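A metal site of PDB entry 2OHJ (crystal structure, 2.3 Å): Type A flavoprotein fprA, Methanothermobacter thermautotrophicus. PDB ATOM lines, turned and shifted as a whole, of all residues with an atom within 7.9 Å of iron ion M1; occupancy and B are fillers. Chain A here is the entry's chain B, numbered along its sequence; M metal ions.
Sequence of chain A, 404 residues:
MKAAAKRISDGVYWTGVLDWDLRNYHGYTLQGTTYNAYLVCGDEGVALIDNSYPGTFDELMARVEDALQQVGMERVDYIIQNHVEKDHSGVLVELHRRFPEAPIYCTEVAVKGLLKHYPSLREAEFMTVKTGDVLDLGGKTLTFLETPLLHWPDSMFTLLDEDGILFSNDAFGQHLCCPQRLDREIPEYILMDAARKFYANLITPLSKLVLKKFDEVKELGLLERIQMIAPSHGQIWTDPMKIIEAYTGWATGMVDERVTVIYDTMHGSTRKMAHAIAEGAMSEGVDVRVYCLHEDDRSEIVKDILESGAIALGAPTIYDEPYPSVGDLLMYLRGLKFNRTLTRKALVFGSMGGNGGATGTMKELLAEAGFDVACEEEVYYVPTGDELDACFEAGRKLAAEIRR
The side-chain carboxylate (OE2) of Glu 85 sits close to the backbone NH (N) of Asp 87, 3.4 Å away.
A ring nitrogen (ND1) of His 233 sits at hydrogen-bond distance from the backbone carbonyl oxygen (O) of Thr 34, at 2.8 Å.
The side-chain amide nitrogen (ND2) of Asn 36 sits close to the backbone NH (N) of His 233, 3.5 Å away.
The side-chain carboxylate (OD1) of Asp 87 lies close to a ring nitrogen (NE2) of His 88, at 2.8 Å.
OD2 of Asp 87 lies within hydrogen-bond range of OH of Tyr 25.
ND1 of His 233 lies within hydrogen-bond range of OG1 of Thr 33 (3.4 Å).
Residues that only touch iron ion M1: Asp 87 (3.5 Å).
Four residues have an atom within 4 Å of iron ion M1: Asp 87, His 88, Asp 170 and His 233.
The side-chain carboxylate (OD1) of Asp 170 is bound to iron ion M1, 2.0 Å away.
Iron ion M1 is bound by a ring nitrogen (NE2) of His 88, 2.1 Å away.
NE2 of His 233 binds iron ion M1.
Iron ion M1 has three donor atoms within binding distance.
Slightly farther from iron ion M1 lies the side-chain carboxylate (OD2) of Asp 170 (2.7 Å).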
ATOM      1  N   TYR A  25      28.502 -22.936  -3.468  1.00  0.00           N
ATOM      2  CA  TYR A  25      27.386 -22.679  -4.398  1.00  0.00           C
ATOM      3  C   TYR A  25      27.868 -21.919  -5.608  1.00  0.00           C
ATOM      4  O   TYR A  25      28.934 -21.305  -5.562  1.00  0.00           O
ATOM      5  CB  TYR A  25      26.198 -21.991  -3.711  1.00  0.00           C
ATOM      6  CG  TYR A  25      26.246 -20.474  -3.561  1.00  0.00           C
ATOM      7  CD1 TYR A  25      25.071 -19.746  -3.588  1.00  0.00           C
ATOM      8  CD2 TYR A  25      27.455 -19.774  -3.377  1.00  0.00           C
ATOM      9  CE1 TYR A  25      25.068 -18.376  -3.440  1.00  0.00           C
ATOM     10  CE2 TYR A  25      27.466 -18.375  -3.243  1.00  0.00           C
ATOM     11  CZ  TYR A  25      26.265 -17.683  -3.277  1.00  0.00           C
ATOM     12  OH  TYR A  25      26.205 -16.323  -3.140  1.00  0.00           O
ATOM     13  N   HIS A  26      27.083 -21.984  -6.694  1.00  0.00           N
ATOM     14  CA  HIS A  26      27.472 -21.383  -7.970  1.00  0.00           C
ATOM     15  C   HIS A  26      28.773 -21.966  -8.542  1.00  0.00           C
ATOM     16  O   HIS A  26      29.419 -21.338  -9.389  1.00  0.00           O
ATOM     17  CB  HIS A  26      27.625 -19.847  -7.831  1.00  0.00           C
ATOM     18  CG  HIS A  26      26.354 -19.120  -7.467  1.00  0.00           C
ATOM     19  ND1 HIS A  26      26.340 -18.003  -6.672  1.00  0.00           N
ATOM     20  CD2 HIS A  26      25.066 -19.368  -7.790  1.00  0.00           C
ATOM     21  CE1 HIS A  26      25.103 -17.573  -6.532  1.00  0.00           C
ATOM     22  NE2 HIS A  26      24.305 -18.383  -7.205  1.00  0.00           N
ATOM     23  N   THR A  33      29.074 -16.249   3.633  1.00  0.00           N
ATOM     24  CA  THR A  33      29.000 -14.987   2.907  1.00  0.00           C
ATOM     25  C   THR A  33      27.947 -14.045   3.520  1.00  0.00           C
ATOM     26  O   THR A  33      27.299 -14.372   4.526  1.00  0.00           O
ATOM     27  CB  THR A  33      28.728 -15.245   1.389  1.00  0.00           C
ATOM     28  OG1 THR A  33      28.766 -14.033   0.641  1.00  0.00           O
ATOM     29  CG2 THR A  33      27.398 -15.976   1.166  1.00  0.00           C
ATOM     30  N   THR A  34      27.831 -12.852   2.956  1.00  0.00           N
ATOM     31  CA  THR A  34      26.762 -11.934   3.314  1.00  0.00           C
ATOM     32  C   THR A  34      25.945 -11.591   2.069  1.00  0.00           C
ATOM     33  O   THR A  34      26.427 -11.687   0.937  1.00  0.00           O
ATOM     34  CB  THR A  34      27.290 -10.656   4.024  1.00  0.00           C
ATOM     35  OG1 THR A  34      27.987  -9.816   3.094  1.00  0.00           O
ATOM     36  CG2 THR A  34      28.237 -11.011   5.163  1.00  0.00           C
ATOM     37  N   TYR A  35      24.685 -11.224   2.303  1.00  0.00           N
ATOM     38  CA  TYR A  35      23.861 -10.584   1.295  1.00  0.00           C
ATOM     39  C   TYR A  35      23.645  -9.177   1.795  1.00  0.00           C
ATOM     40  O   TYR A  35      22.848  -8.951   2.697  1.00  0.00           O
ATOM     41  CB  TYR A  35      22.533 -11.331   1.090  1.00  0.00           C
ATOM     42  CG  TYR A  35      22.749 -12.810   1.045  1.00  0.00           C
ATOM     43  CD1 TYR A  35      23.553 -13.380   0.049  1.00  0.00           C
ATOM     44  CD2 TYR A  35      22.187 -13.675   2.020  1.00  0.00           C
ATOM     45  CE1 TYR A  35      23.781 -14.726   0.009  1.00  0.00           C
ATOM     46  CE2 TYR A  35      22.430 -15.026   1.972  1.00  0.00           C
ATOM     47  CZ  TYR A  35      23.235 -15.547   0.965  1.00  0.00           C
ATOM     48  OH  TYR A  35      23.500 -16.888   0.881  1.00  0.00           O
ATOM     49  N   ASN A  36      24.415  -8.257   1.221  1.00  0.00           N
ATOM     50  CA  ASN A  36      24.422  -6.860   1.666  1.00  0.00           C
ATOM     51  C   ASN A  36      23.232  -6.103   1.094  1.00  0.00           C
ATOM     52  O   ASN A  36      22.995  -6.106  -0.119  1.00  0.00           O
ATOM     53  CB  ASN A  36      25.745  -6.179   1.315  1.00  0.00           C
ATOM     54  CG  ASN A  36      26.941  -6.803   2.025  1.00  0.00           C
ATOM     55  OD1 ASN A  36      26.802  -7.362   3.126  1.00  0.00           O
ATOM     56  ND2 ASN A  36      28.137  -6.704   1.425  1.00  0.00           N
ATOM     57  N   HIS A  83      20.021  -6.163  -9.054  1.00  0.00           N
ATOM     58  CA  HIS A  83      20.059  -7.444  -9.782  1.00  0.00           C
ATOM     59  C   HIS A  83      18.940  -8.407  -9.382  1.00  0.00           C
ATOM     60  O   HIS A  83      18.374  -8.287  -8.291  1.00  0.00           O
ATOM     61  CB  HIS A  83      21.431  -8.160  -9.756  1.00  0.00           C
ATOM     62  CG  HIS A  83      22.193  -8.011  -8.479  1.00  0.00           C
ATOM     63  ND1 HIS A  83      21.755  -7.237  -7.416  1.00  0.00           N
ATOM     64  CD2 HIS A  83      23.398  -8.518  -8.099  1.00  0.00           C
ATOM     65  CE1 HIS A  83      22.658  -7.280  -6.447  1.00  0.00           C
ATOM     66  NE2 HIS A  83      23.668  -8.046  -6.847  1.00  0.00           N
ATOM     67  N   GLU A  85      19.312 -11.880  -9.328  1.00  0.00           N
ATOM     68  CA  GLU A  85      19.876 -13.079  -8.669  1.00  0.00           C
ATOM     69  C   GLU A  85      19.242 -13.317  -7.283  1.00  0.00           C
ATOM     70  O   GLU A  85      19.179 -12.397  -6.455  1.00  0.00           O
ATOM     71  CB  GLU A  85      21.411 -12.977  -8.589  1.00  0.00           C
ATOM     72  CG  GLU A  85      22.074 -13.621  -7.383  1.00  0.00           C
ATOM     73  CD  GLU A  85      22.300 -15.122  -7.561  1.00  0.00           C
ATOM     74  OE1 GLU A  85      22.755 -15.556  -8.649  1.00  0.00           O
ATOM     75  OE2 GLU A  85      22.050 -15.870  -6.582  1.00  0.00           O
ATOM     76  N   LYS A  86      18.776 -14.551  -7.068  1.00  0.00           N
ATOM     77  CA  LYS A  86      17.916 -14.894  -5.918  1.00  0.00           C
ATOM     78  C   LYS A  86      18.521 -14.585  -4.551  1.00  0.00           C
ATOM     79  O   LYS A  86      17.790 -14.434  -3.576  1.00  0.00           O
ATOM     80  CB  LYS A  86      17.397 -16.347  -5.992  1.00  0.00           C
ATOM     81  CG  LYS A  86      18.360 -17.420  -5.513  1.00  0.00           C
ATOM     82  CD  LYS A  86      17.821 -18.850  -5.722  1.00  0.00           C
ATOM     83  CE  LYS A  86      16.790 -19.279  -4.667  1.00  0.00           C
ATOM     84  NZ  LYS A  86      16.204 -20.660  -4.947  1.00  0.00           N
ATOM     85  N   ASP A  87      19.840 -14.494  -4.441  1.00  0.00           N
ATOM     86  CA  ASP A  87      20.348 -14.131  -3.141  1.00  0.00           C
ATOM     87  C   ASP A  87      20.312 -12.647  -2.805  1.00  0.00           C
ATOM     88  O   ASP A  87      20.560 -12.256  -1.673  1.00  0.00           O
ATOM     89  CB  ASP A  87      21.635 -14.889  -2.737  1.00  0.00           C
ATOM     90  CG  ASP A  87      22.789 -14.632  -3.623  1.00  0.00           C
ATOM     91  OD1 ASP A  87      22.850 -13.529  -4.198  1.00  0.00           O
ATOM     92  OD2 ASP A  87      23.675 -15.498  -3.723  1.00  0.00           O
ATOM     93  N   HIS A  88      19.856 -11.836  -3.785  1.00  0.00           N
ATOM     94  CA  HIS A  88      19.620 -10.393  -3.602  1.00  0.00           C
ATOM     95  C   HIS A  88      18.171  -9.962  -3.878  1.00  0.00           C
ATOM     96  O   HIS A  88      17.801  -8.806  -3.606  1.00  0.00           O
ATOM     97  CB  HIS A  88      20.585  -9.570  -4.458  1.00  0.00           C
ATOM     98  CG  HIS A  88      21.983 -10.096  -4.418  1.00  0.00           C
ATOM     99  ND1 HIS A  88      22.760 -10.039  -3.286  1.00  0.00           N
ATOM    100  CD2 HIS A  88      22.733 -10.730  -5.355  1.00  0.00           C
ATOM    101  CE1 HIS A  88      23.928 -10.601  -3.525  1.00  0.00           C
ATOM    102  NE2 HIS A  88      23.937 -11.034  -4.771  1.00  0.00           N
ATOM    103  N   TRP A 152      25.536 -10.338 -17.141  1.00  0.00           N
ATOM    104  CA  TRP A 152      24.730  -9.918 -15.987  1.00  0.00           C
ATOM    105  C   TRP A 152      23.681  -8.933 -16.510  1.00  0.00           C
ATOM    106  O   TRP A 152      23.656  -7.772 -16.079  1.00  0.00           O
ATOM    107  CB  TRP A 152      25.609  -9.200 -14.987  1.00  0.00           C
ATOM    108  CG  TRP A 152      26.731  -9.986 -14.374  1.00  0.00           C
ATOM    109  CD1 TRP A 152      27.122 -11.248 -14.695  1.00  0.00           C
ATOM    110  CD2 TRP A 152      27.617  -9.531 -13.340  1.00  0.00           C
ATOM    111  NE1 TRP A 152      28.199 -11.624 -13.911  1.00  0.00           N
ATOM    112  CE2 TRP A 152      28.521 -10.584 -13.074  1.00  0.00           C
ATOM    113  CE3 TRP A 152      27.738  -8.346 -12.609  1.00  0.00           C
ATOM    114  CZ2 TRP A 152      29.538 -10.487 -12.106  1.00  0.00           C
ATOM    115  CZ3 TRP A 152      28.754  -8.245 -11.632  1.00  0.00           C
ATOM    116  CH2 TRP A 152      29.633  -9.306 -11.397  1.00  0.00           C
ATOM    117  N   ASN A 169      26.431  -3.804  -6.823  1.00  0.00           N
ATOM    118  CA  ASN A 169      25.971  -5.193  -6.989  1.00  0.00           C
ATOM    119  C   ASN A 169      27.124  -6.187  -6.686  1.00  0.00           C
ATOM    120  O   ASN A 169      27.875  -5.944  -5.730  1.00  0.00           O
ATOM    121  CB  ASN A 169      25.147  -5.426  -8.310  1.00  0.00           C
ATOM    122  CG  ASN A 169      25.993  -5.402  -9.633  1.00  0.00           C
ATOM    123  OD1 ASN A 169      26.751  -6.339  -9.919  1.00  0.00           O
ATOM    124  ND2 ASN A 169      25.781  -4.394 -10.463  1.00  0.00           N
ATOM    125  N   ASP A 170      27.303  -7.262  -7.432  1.00  0.00           N
ATOM    126  CA  ASP A 170      28.358  -8.234  -7.124  1.00  0.00           C
ATOM    127  C   ASP A 170      29.790  -7.742  -7.423  1.00  0.00           C
ATOM    128  O   ASP A 170      30.740  -8.283  -6.871  1.00  0.00           O
ATOM    129  CB  ASP A 170      28.154  -9.560  -7.874  1.00  0.00           C
ATOM    130  CG  ASP A 170      27.021 -10.418  -7.281  1.00  0.00           C
ATOM    131  OD1 ASP A 170      26.661 -10.322  -6.094  1.00  0.00           O
ATOM    132  OD2 ASP A 170      26.484 -11.232  -8.052  1.00  0.00           O
ATOM    133  N   ALA A 171      29.930  -6.728  -8.281  1.00  0.00           N
ATOM    134  CA  ALA A 171      31.266  -6.197  -8.573  1.00  0.00           C
ATOM    135  C   ALA A 171      31.939  -5.767  -7.257  1.00  0.00           C
ATOM    136  O   ALA A 171      31.292  -5.201  -6.390  1.00  0.00           O
ATOM    137  CB  ALA A 171      31.197  -5.010  -9.551  1.00  0.00           C
ATOM    138  N   GLY A 173      32.730  -7.553  -4.889  1.00  0.00           N
ATOM    139  CA  GLY A 173      32.284  -8.418  -3.827  1.00  0.00           C
ATOM    140  C   GLY A 173      33.370  -9.400  -3.402  1.00  0.00           C
ATOM    141  O   GLY A 173      34.407  -9.565  -4.069  1.00  0.00           O
ATOM    142  N   HIS A 175      33.218 -13.246  -0.906  1.00  0.00           N
ATOM    143  CA  HIS A 175      32.436 -14.141  -0.034  1.00  0.00           C
ATOM    144  C   HIS A 175      33.090 -14.288   1.327  1.00  0.00           C
ATOM    145  O   HIS A 175      33.952 -15.141   1.541  1.00  0.00           O
ATOM    146  CB  HIS A 175      32.139 -15.488  -0.715  1.00  0.00           C
ATOM    147  CG  HIS A 175      31.239 -15.349  -1.894  1.00  0.00           C
ATOM    148  ND1 HIS A 175      29.930 -14.926  -1.768  1.00  0.00           N
ATOM    149  CD2 HIS A 175      31.457 -15.514  -3.215  1.00  0.00           C
ATOM    150  CE1 HIS A 175      29.385 -14.859  -2.972  1.00  0.00           C
ATOM    151  NE2 HIS A 175      30.291 -15.214  -3.860  1.00  0.00           N
ATOM    152  N   PHE A 198      36.898 -14.121  -5.935  1.00  0.00           N
ATOM    153  CA  PHE A 198      35.636 -13.648  -6.502  1.00  0.00           C
ATOM    154  C   PHE A 198      35.895 -13.161  -7.936  1.00  0.00           C
ATOM    155  O   PHE A 198      35.122 -13.473  -8.861  1.00  0.00           O
ATOM    156  CB  PHE A 198      35.102 -12.504  -5.630  1.00  0.00           C
ATOM    157  CG  PHE A 198      33.646 -12.216  -5.807  1.00  0.00           C
ATOM    158  CD1 PHE A 198      32.711 -12.762  -4.933  1.00  0.00           C
ATOM    159  CD2 PHE A 198      33.208 -11.345  -6.802  1.00  0.00           C
ATOM    160  CE1 PHE A 198      31.343 -12.461  -5.054  1.00  0.00           C
ATOM    161  CE2 PHE A 198      31.858 -11.045  -6.953  1.00  0.00           C
ATOM    162  CZ  PHE A 198      30.913 -11.609  -6.072  1.00  0.00           C
ATOM    163  N   LEU A 202      34.268 -15.161 -11.066  1.00  0.00           N
ATOM    164  CA  LEU A 202      33.051 -14.452 -11.508  1.00  0.00           C
ATOM    165  C   LEU A 202      33.255 -13.303 -12.512  1.00  0.00           C
ATOM    166  O   LEU A 202      32.347 -12.971 -13.262  1.00  0.00           O
ATOM    167  CB  LEU A 202      32.231 -14.003 -10.280  1.00  0.00           C
ATOM    168  CG  LEU A 202      31.845 -15.172  -9.337  1.00  0.00           C
ATOM    169  CD1 LEU A 202      31.375 -14.718  -7.983  1.00  0.00           C
ATOM    170  CD2 LEU A 202      30.783 -16.086  -9.983  1.00  0.00           C
ATOM    171  N   PRO A 231      29.540  -3.319  -1.858  1.00  0.00           N
ATOM    172  CA  PRO A 231      29.159  -4.419  -2.750  1.00  0.00           C
ATOM    173  C   PRO A 231      28.063  -5.312  -2.148  1.00  0.00           C
ATOM    174  O   PRO A 231      27.708  -5.122  -0.994  1.00  0.00           O
ATOM    175  CB  PRO A 231      30.482  -5.179  -2.917  1.00  0.00           C
ATOM    176  CG  PRO A 231      31.159  -4.985  -1.613  1.00  0.00           C
ATOM    177  CD  PRO A 231      30.760  -3.625  -1.095  1.00  0.00           C
ATOM    178  N   SER A 232      27.568  -6.286  -2.920  1.00  0.00           N
ATOM    179  CA  SER A 232      26.469  -7.145  -2.456  1.00  0.00           C
ATOM    180  C   SER A 232      26.890  -8.323  -1.552  1.00  0.00           C
ATOM    181  O   SER A 232      26.044  -8.981  -0.940  1.00  0.00           O
ATOM    182  CB  SER A 232      25.641  -7.644  -3.631  1.00  0.00           C
ATOM    183  OG  SER A 232      24.801  -6.611  -4.104  1.00  0.00           O
ATOM    184  N   HIS A 233      28.193  -8.577  -1.481  1.00  0.00           N
ATOM    185  CA  HIS A 233      28.730  -9.589  -0.557  1.00  0.00           C
ATOM    186  C   HIS A 233      29.969  -9.072   0.113  1.00  0.00           C
ATOM    187  O   HIS A 233      30.779  -8.383  -0.517  1.00  0.00           O
ATOM    188  CB  HIS A 233      29.148 -10.875  -1.273  1.00  0.00           C
ATOM    189  CG  HIS A 233      28.095 -11.438  -2.171  1.00  0.00           C
ATOM    190  ND1 HIS A 233      27.120 -12.309  -1.725  1.00  0.00           N
ATOM    191  CD2 HIS A 233      27.880 -11.267  -3.496  1.00  0.00           C
ATOM    192  CE1 HIS A 233      26.369 -12.669  -2.747  1.00  0.00           C
ATOM    193  NE2 HIS A 233      26.803 -12.054  -3.828  1.00  0.00           N
HETATM  194 FE    FE M   1      25.612 -11.946  -5.602  1.00  0.00          FE
HETATM  195 FE    FE M   2      22.294 -17.855  -6.722  1.00  0.00          FE
